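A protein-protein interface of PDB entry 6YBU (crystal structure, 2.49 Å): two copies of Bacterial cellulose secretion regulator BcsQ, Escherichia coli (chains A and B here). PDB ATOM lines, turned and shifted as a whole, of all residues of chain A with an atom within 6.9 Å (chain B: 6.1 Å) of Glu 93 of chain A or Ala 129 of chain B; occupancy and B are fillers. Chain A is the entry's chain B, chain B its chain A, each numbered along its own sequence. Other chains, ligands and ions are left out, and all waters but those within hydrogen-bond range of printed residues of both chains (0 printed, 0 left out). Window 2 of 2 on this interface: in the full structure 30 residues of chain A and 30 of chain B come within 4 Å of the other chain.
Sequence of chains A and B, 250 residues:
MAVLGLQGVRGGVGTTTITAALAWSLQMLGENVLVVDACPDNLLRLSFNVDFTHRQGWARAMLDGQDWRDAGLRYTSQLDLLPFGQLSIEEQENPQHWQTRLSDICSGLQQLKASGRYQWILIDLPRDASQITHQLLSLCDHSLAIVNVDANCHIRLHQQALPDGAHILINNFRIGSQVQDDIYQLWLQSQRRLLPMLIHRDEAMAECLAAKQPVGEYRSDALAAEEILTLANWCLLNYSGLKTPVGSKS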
ATOM      1  N   SER A  88     -28.269 -30.005  13.995  1.00  0.00           N
ATOM      2  CA  SER A  88     -28.416 -28.559  14.018  1.00  0.00           C
ATOM      3  C   SER A  88     -27.267 -27.932  14.804  1.00  0.00           C
ATOM      4  O   SER A  88     -26.500 -28.613  15.490  1.00  0.00           O
ATOM      5  CB  SER A  88     -29.762 -28.161  14.621  1.00  0.00           C
ATOM      6  OG  SER A  88     -29.807 -28.447  16.008  1.00  0.00           O
ATOM      7  N   ILE A  89     -27.150 -26.606  14.694  1.00  0.00           N
ATOM      8  CA  ILE A  89     -26.073 -25.901  15.383  1.00  0.00           C
ATOM      9  C   ILE A  89     -26.192 -26.082  16.892  1.00  0.00           C
ATOM     10  O   ILE A  89     -25.189 -26.293  17.585  1.00  0.00           O
ATOM     11  CB  ILE A  89     -26.059 -24.414  14.982  1.00  0.00           C
ATOM     12  CG1 ILE A  89     -25.474 -24.253  13.577  1.00  0.00           C
ATOM     13  CG2 ILE A  89     -25.274 -23.586  15.989  1.00  0.00           C
ATOM     14  CD1 ILE A  89     -25.280 -22.813  13.152  1.00  0.00           C
ATOM     15  N   GLU A  90     -27.418 -26.030  17.423  1.00  0.00           N
ATOM     16  CA  GLU A  90     -27.607 -26.242  18.856  1.00  0.00           C
ATOM     17  C   GLU A  90     -27.148 -27.635  19.271  1.00  0.00           C
ATOM     18  O   GLU A  90     -26.449 -27.795  20.278  1.00  0.00           O
ATOM     19  CB  GLU A  90     -29.069 -26.024  19.247  1.00  0.00           C
ATOM     20  CG  GLU A  90     -29.404 -26.603  20.618  1.00  0.00           C
ATOM     21  CD  GLU A  90     -30.732 -26.121  21.166  1.00  0.00           C
ATOM     22  OE1 GLU A  90     -31.261 -25.111  20.656  1.00  0.00           O
ATOM     23  OE2 GLU A  90     -31.244 -26.757  22.113  1.00  0.00           O
ATOM     24  N   GLU A  91     -27.532 -28.656  18.502  1.00  0.00           N
ATOM     25  CA  GLU A  91     -27.101 -30.016  18.817  1.00  0.00           C
ATOM     26  C   GLU A  91     -25.584 -30.141  18.745  1.00  0.00           C
ATOM     27  O   GLU A  91     -24.971 -30.832  19.568  1.00  0.00           O
ATOM     28  CB  GLU A  91     -27.767 -31.014  17.871  1.00  0.00           C
ATOM     29  CG  GLU A  91     -29.284 -30.980  17.898  1.00  0.00           C
ATOM     30  CD  GLU A  91     -29.906 -31.867  16.836  1.00  0.00           C
ATOM     31  OE1 GLU A  91     -30.567 -32.866  17.199  1.00  0.00           O
ATOM     32  OE2 GLU A  91     -29.729 -31.569  15.634  1.00  0.00           O
ATOM     33  N   GLN A  92     -24.962 -29.472  17.769  1.00  0.00           N
ATOM     34  CA  GLN A  92     -23.505 -29.483  17.673  1.00  0.00           C
ATOM     35  C   GLN A  92     -22.866 -28.852  18.904  1.00  0.00           C
ATOM     36  O   GLN A  92     -21.864 -29.360  19.422  1.00  0.00           O
ATOM     37  CB  GLN A  92     -23.056 -28.749  16.410  1.00  0.00           C
ATOM     38  CG  GLN A  92     -23.440 -29.426  15.106  1.00  0.00           C
ATOM     39  CD  GLN A  92     -23.060 -28.593  13.898  1.00  0.00           C
ATOM     40  OE1 GLN A  92     -22.146 -27.771  13.959  1.00  0.00           O
ATOM     41  NE2 GLN A  92     -23.770 -28.793  12.794  1.00  0.00           N
ATOM     42  N   GLU A  93     -23.431 -27.745  19.390  1.00  0.00           N
ATOM     43  CA  GLU A  93     -22.844 -27.042  20.523  1.00  0.00           C
ATOM     44  C   GLU A  93     -23.123 -27.727  21.854  1.00  0.00           C
ATOM     45  O   GLU A  93     -22.385 -27.496  22.818  1.00  0.00           O
ATOM     46  CB  GLU A  93     -23.354 -25.598  20.578  1.00  0.00           C
ATOM     47  CG  GLU A  93     -23.075 -24.784  19.321  1.00  0.00           C
ATOM     48  CD  GLU A  93     -21.602 -24.735  18.958  1.00  0.00           C
ATOM     49  OE1 GLU A  93     -20.754 -24.776  19.874  1.00  0.00           O
ATOM     50  OE2 GLU A  93     -21.293 -24.657  17.750  1.00  0.00           O
ATOM     51  N   ASN A  94     -24.157 -28.562  21.932  1.00  0.00           N
ATOM     52  CA  ASN A  94     -24.547 -29.232  23.173  1.00  0.00           C
ATOM     53  C   ASN A  94     -24.622 -30.736  22.936  1.00  0.00           C
ATOM     54  O   ASN A  94     -25.714 -31.309  22.835  1.00  0.00           O
ATOM     55  CB  ASN A  94     -25.882 -28.691  23.691  1.00  0.00           C
ATOM     56  CG  ASN A  94     -25.849 -27.193  23.925  1.00  0.00           C
ATOM     57  OD1 ASN A  94     -25.543 -26.732  25.024  1.00  0.00           O
ATOM     58  ND2 ASN A  94     -26.160 -26.425  22.886  1.00  0.00           N
ATOM     59  N   PRO A  95     -23.472 -31.409  22.852  1.00  0.00           N
ATOM     60  CA  PRO A  95     -23.491 -32.865  22.624  1.00  0.00           C
ATOM     61  C   PRO A  95     -24.178 -33.645  23.732  1.00  0.00           C
ATOM     62  O   PRO A  95     -24.769 -34.698  23.457  1.00  0.00           O
ATOM     63  CB  PRO A  95     -22.001 -33.223  22.520  1.00  0.00           C
ATOM     64  CG  PRO A  95     -21.283 -32.106  23.203  1.00  0.00           C
ATOM     65  CD  PRO A  95     -22.101 -30.880  22.939  1.00  0.00           C
ATOM     66  N   GLN A  96     -24.130 -33.160  24.976  1.00  0.00           N
ATOM     67  CA  GLN A  96     -24.775 -33.871  26.074  1.00  0.00           C
ATOM     68  C   GLN A  96     -26.286 -33.950  25.907  1.00  0.00           C
ATOM     69  O   GLN A  96     -26.931 -34.757  26.585  1.00  0.00           O
ATOM     70  CB  GLN A  96     -24.431 -33.205  27.407  1.00  0.00           C
ATOM     71  CG  GLN A  96     -22.963 -33.313  27.788  1.00  0.00           C
ATOM     72  CD  GLN A  96     -22.686 -32.833  29.204  1.00  0.00           C
ATOM     73  OE1 GLN A  96     -23.558 -32.265  29.863  1.00  0.00           O
ATOM     74  NE2 GLN A  96     -21.465 -33.065  29.680  1.00  0.00           N
ATOM     75  N   TRP A  98     -27.800 -34.978  23.154  1.00  0.00           N
ATOM     76  CA  TRP A  98     -28.133 -36.082  22.267  1.00  0.00           C
ATOM     77  C   TRP A  98     -27.190 -37.275  22.354  1.00  0.00           C
ATOM     78  O   TRP A  98     -27.538 -38.345  21.844  1.00  0.00           O
ATOM     79  CB  TRP A  98     -28.177 -35.600  20.808  1.00  0.00           C
ATOM     80  CG  TRP A  98     -26.941 -34.872  20.376  1.00  0.00           C
ATOM     81  CD1 TRP A  98     -26.758 -33.520  20.338  1.00  0.00           C
ATOM     82  CD2 TRP A  98     -25.710 -35.453  19.926  1.00  0.00           C
ATOM     83  NE1 TRP A  98     -25.493 -33.224  19.893  1.00  0.00           N
ATOM     84  CE2 TRP A  98     -24.830 -34.393  19.632  1.00  0.00           C
ATOM     85  CE3 TRP A  98     -25.267 -36.766  19.744  1.00  0.00           C
ATOM     86  CZ2 TRP A  98     -23.535 -34.606  19.163  1.00  0.00           C
ATOM     87  CZ3 TRP A  98     -23.981 -36.976  19.277  1.00  0.00           C
ATOM     88  CH2 TRP A  98     -23.131 -35.902  18.990  1.00  0.00           C
ATOM     89  N   GLN B  99     -14.443 -32.216  33.174  1.00  0.00           N
ATOM     90  CA  GLN B  99     -14.752 -31.088  32.300  1.00  0.00           C
ATOM     91  C   GLN B  99     -15.731 -30.101  32.926  1.00  0.00           C
ATOM     92  O   GLN B  99     -16.037 -29.079  32.300  1.00  0.00           O
ATOM     93  CB  GLN B  99     -15.293 -31.583  30.956  1.00  0.00           C
ATOM     94  CG  GLN B  99     -16.783 -31.869  30.924  1.00  0.00           C
ATOM     95  CD  GLN B  99     -17.297 -32.074  29.511  1.00  0.00           C
ATOM     96  OE1 GLN B  99     -16.629 -32.688  28.678  1.00  0.00           O
ATOM     97  NE2 GLN B  99     -18.483 -31.547  29.230  1.00  0.00           N
ATOM     98  N   ARG B 127     -11.684 -27.795  19.539  1.00  0.00           N
ATOM     99  CA  ARG B 127     -12.964 -27.673  18.854  1.00  0.00           C
ATOM    100  C   ARG B 127     -14.021 -28.616  19.427  1.00  0.00           C
ATOM    101  O   ARG B 127     -15.060 -28.835  18.799  1.00  0.00           O
ATOM    102  CB  ARG B 127     -12.769 -27.902  17.348  1.00  0.00           C
ATOM    103  CG  ARG B 127     -13.962 -27.564  16.426  1.00  0.00           C
ATOM    104  CD  ARG B 127     -14.706 -26.292  16.829  1.00  0.00           C
ATOM    105  NE  ARG B 127     -15.968 -26.150  16.099  1.00  0.00           N
ATOM    106  CZ  ARG B 127     -17.162 -26.474  16.590  1.00  0.00           C
ATOM    107  NH1 ARG B 127     -17.266 -26.952  17.823  1.00  0.00           N
ATOM    108  NH2 ARG B 127     -18.253 -26.315  15.852  1.00  0.00           N
ATOM    109  N   ASP B 128     -13.795 -29.171  20.615  1.00  0.00           N
ATOM    110  CA  ASP B 128     -14.891 -29.859  21.279  1.00  0.00           C
ATOM    111  C   ASP B 128     -15.955 -28.837  21.690  1.00  0.00           C
ATOM    112  O   ASP B 128     -15.785 -27.624  21.540  1.00  0.00           O
ATOM    113  CB  ASP B 128     -14.383 -30.670  22.474  1.00  0.00           C
ATOM    114  CG  ASP B 128     -13.662 -29.821  23.512  1.00  0.00           C
ATOM    115  OD1 ASP B 128     -13.809 -28.583  23.505  1.00  0.00           O
ATOM    116  OD2 ASP B 128     -12.933 -30.404  24.341  1.00  0.00           O
ATOM    117  N   ALA B 129     -17.073 -29.329  22.214  1.00  0.00           N
ATOM    118  CA  ALA B 129     -18.165 -28.461  22.633  1.00  0.00           C
ATOM    119  C   ALA B 129     -18.383 -28.520  24.142  1.00  0.00           C
ATOM    120  O   ALA B 129     -19.504 -28.336  24.620  1.00  0.00           O
ATOM    121  CB  ALA B 129     -19.450 -28.810  21.886  1.00  0.00           C
ATOM    122  N   SER B 130     -17.319 -28.772  24.900  1.00  0.00           N
ATOM    123  CA  SER B 130     -17.425 -28.823  26.350  1.00  0.00           C
ATOM    124  C   SER B 130     -17.712 -27.434  26.913  1.00  0.00           C
ATOM    125  O   SER B 130     -17.402 -26.409  26.300  1.00  0.00           O
ATOM    126  CB  SER B 130     -16.142 -29.385  26.964  1.00  0.00           C
ATOM    127  OG  SER B 130     -15.039 -28.528  26.717  1.00  0.00           O
ATOM    128  N   GLN B 131     -18.312 -27.413  28.107  1.00  0.00           N
ATOM    129  CA  GLN B 131     -18.692 -26.141  28.715  1.00  0.00           C
ATOM    130  C   GLN B 131     -17.476 -25.276  29.024  1.00  0.00           C
ATOM    131  O   GLN B 131     -17.551 -24.047  28.925  1.00  0.00           O
ATOM    132  CB  GLN B 131     -19.513 -26.383  29.985  1.00  0.00           C
ATOM    133  CG  GLN B 131     -18.756 -27.055  31.121  1.00  0.00           C
ATOM    134  CD  GLN B 131     -19.531 -27.033  32.425  1.00  0.00           C
ATOM    135  OE1 GLN B 131     -18.956 -27.152  33.507  1.00  0.00           O
ATOM    136  NE2 GLN B 131     -20.846 -26.877  32.328  1.00  0.00           N
ATOM    137  N   THR B 133     -14.738 -25.159  27.278  1.00  0.00           N
ATOM    138  CA  THR B 133     -14.269 -24.582  26.021  1.00  0.00           C
ATOM    139  C   THR B 133     -15.087 -23.355  25.639  1.00  0.00           C
ATOM    140  O   THR B 133     -14.529 -22.337  25.212  1.00  0.00           O
ATOM    141  CB  THR B 133     -14.319 -25.631  24.910  1.00  0.00           C
ATOM    142  OG1 THR B 133     -13.386 -26.682  25.193  1.00  0.00           O
ATOM    143  CG2 THR B 133     -13.978 -25.007  23.564  1.00  0.00           C
ATOM    144  N   HIS B 134     -16.413 -23.431  25.790  1.00  0.00           N
ATOM    145  CA  HIS B 134     -17.261 -22.287  25.465  1.00  0.00           C
ATOM    146  C   HIS B 134     -17.012 -21.124  26.418  1.00  0.00           C
ATOM    147  O   HIS B 134     -17.067 -19.958  26.007  1.00  0.00           O
ATOM    148  CB  HIS B 134     -18.732 -22.698  25.496  1.00  0.00           C
ATOM    149  CG  HIS B 134     -19.148 -23.545  24.334  1.00  0.00           C
ATOM    150  ND1 HIS B 134     -19.936 -24.667  24.475  1.00  0.00           N
ATOM    151  CD2 HIS B 134     -18.895 -23.428  23.009  1.00  0.00           C
ATOM    152  CE1 HIS B 134     -20.144 -25.209  23.288  1.00  0.00           C
ATOM    153  NE2 HIS B 134     -19.523 -24.476  22.381  1.00  0.00           N
ATOM    154  N   GLN B 160     -20.904 -25.829  10.090  1.00  0.00           N
ATOM    155  CA  GLN B 160     -20.632 -25.640  11.508  1.00  0.00           C
ATOM    156  C   GLN B 160     -20.416 -24.159  11.790  1.00  0.00           C
ATOM    157  O   GLN B 160     -20.212 -23.350  10.880  1.00  0.00           O
ATOM    158  CB  GLN B 160     -19.419 -26.462  11.972  1.00  0.00           C
ATOM    159  CG  GLN B 160     -18.071 -25.861  11.625  1.00  0.00           C
ATOM    160  CD  GLN B 160     -16.927 -26.809  11.920  1.00  0.00           C
ATOM    161  OE1 GLN B 160     -17.043 -28.018  11.724  1.00  0.00           O
ATOM    162  NE2 GLN B 160     -15.814 -26.264  12.401  1.00  0.00           N
ATOM    163  N   ALA B 161     -20.466 -23.810  13.072  1.00  0.00           N
ATOM    164  CA  ALA B 161     -20.388 -22.425  13.510  1.00  0.00           C
ATOM    165  C   ALA B 161     -18.962 -22.064  13.902  1.00  0.00           C
ATOM    166  O   ALA B 161     -18.257 -22.856  14.536  1.00  0.00           O
ATOM    167  CB  ALA B 161     -21.326 -22.173  14.691  1.00  0.00           C
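Along chain A the printed residues that touch a printed residue of chain B span positions 92 to 96. Hydrophobic or aromatic side chains of chain B that line the printed part of chain A: Ala 129, His 134 and Ala 161. Among the printed residues, 8 pairs touch across the chains.
Glu 90 of chain A touches none of the printed residues of chain B. Glu 91 of chain A touches none of the printed residues of chain B. Of the printed residues of chain B, Gln 92 of chain A touches Ala 129 and Gln 160. Glu 93 of chain A touches four residues of chain B. Printed residues of chain B within 4 Å of Gln 96 of chain A: Gln 99 (3.4 Å). Printed residues of chain A within 4 Å of Arg 127 of chain B: Glu 93 (3.9 Å). Ala 129 of chain B touches three residues of chain A. Printed residues of chain A within 4 Å of Ala 161 of chain B: Glu 93. The nearest residue of chain A that does not touch Ala 129 of chain B is Asn 94 of chain A (4.7 Å).
The side-chain amide nitrogen of Gln 99 of chain B lies close to the side-chain amide nitrogen of Gln 96 of chain A (3.4 Å). A ring nitrogen (NE2) of His 134 of chain B is in hydrogen-bond range of the side-chain carboxylate (OE1) of Glu 93 of chain A (2.8 Å). NH2 of Arg 127 of chain B is in salt-bridge range of OE2 of Glu 93 of chain A (3.9 Å).
Gln 92 of chain A touches Ala 129 of chain B (O to CB, 3.5 Å). Gln 160 of chain B touches Gln 92 of chain A. CB of Ala 129 of chain B touches O of Glu 93 of chain A, at 3.3 Å. Glu 93 of chain A touches Ala 161 of chain B. Pro 95 of chain A touches Ala 129 of chain B (CD to CB, 3.5 Å).
No position is printed for both chains. Of the 8 pairs that touch across the chains among the printed residues, none has its exchanged pair printed and touching as well.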
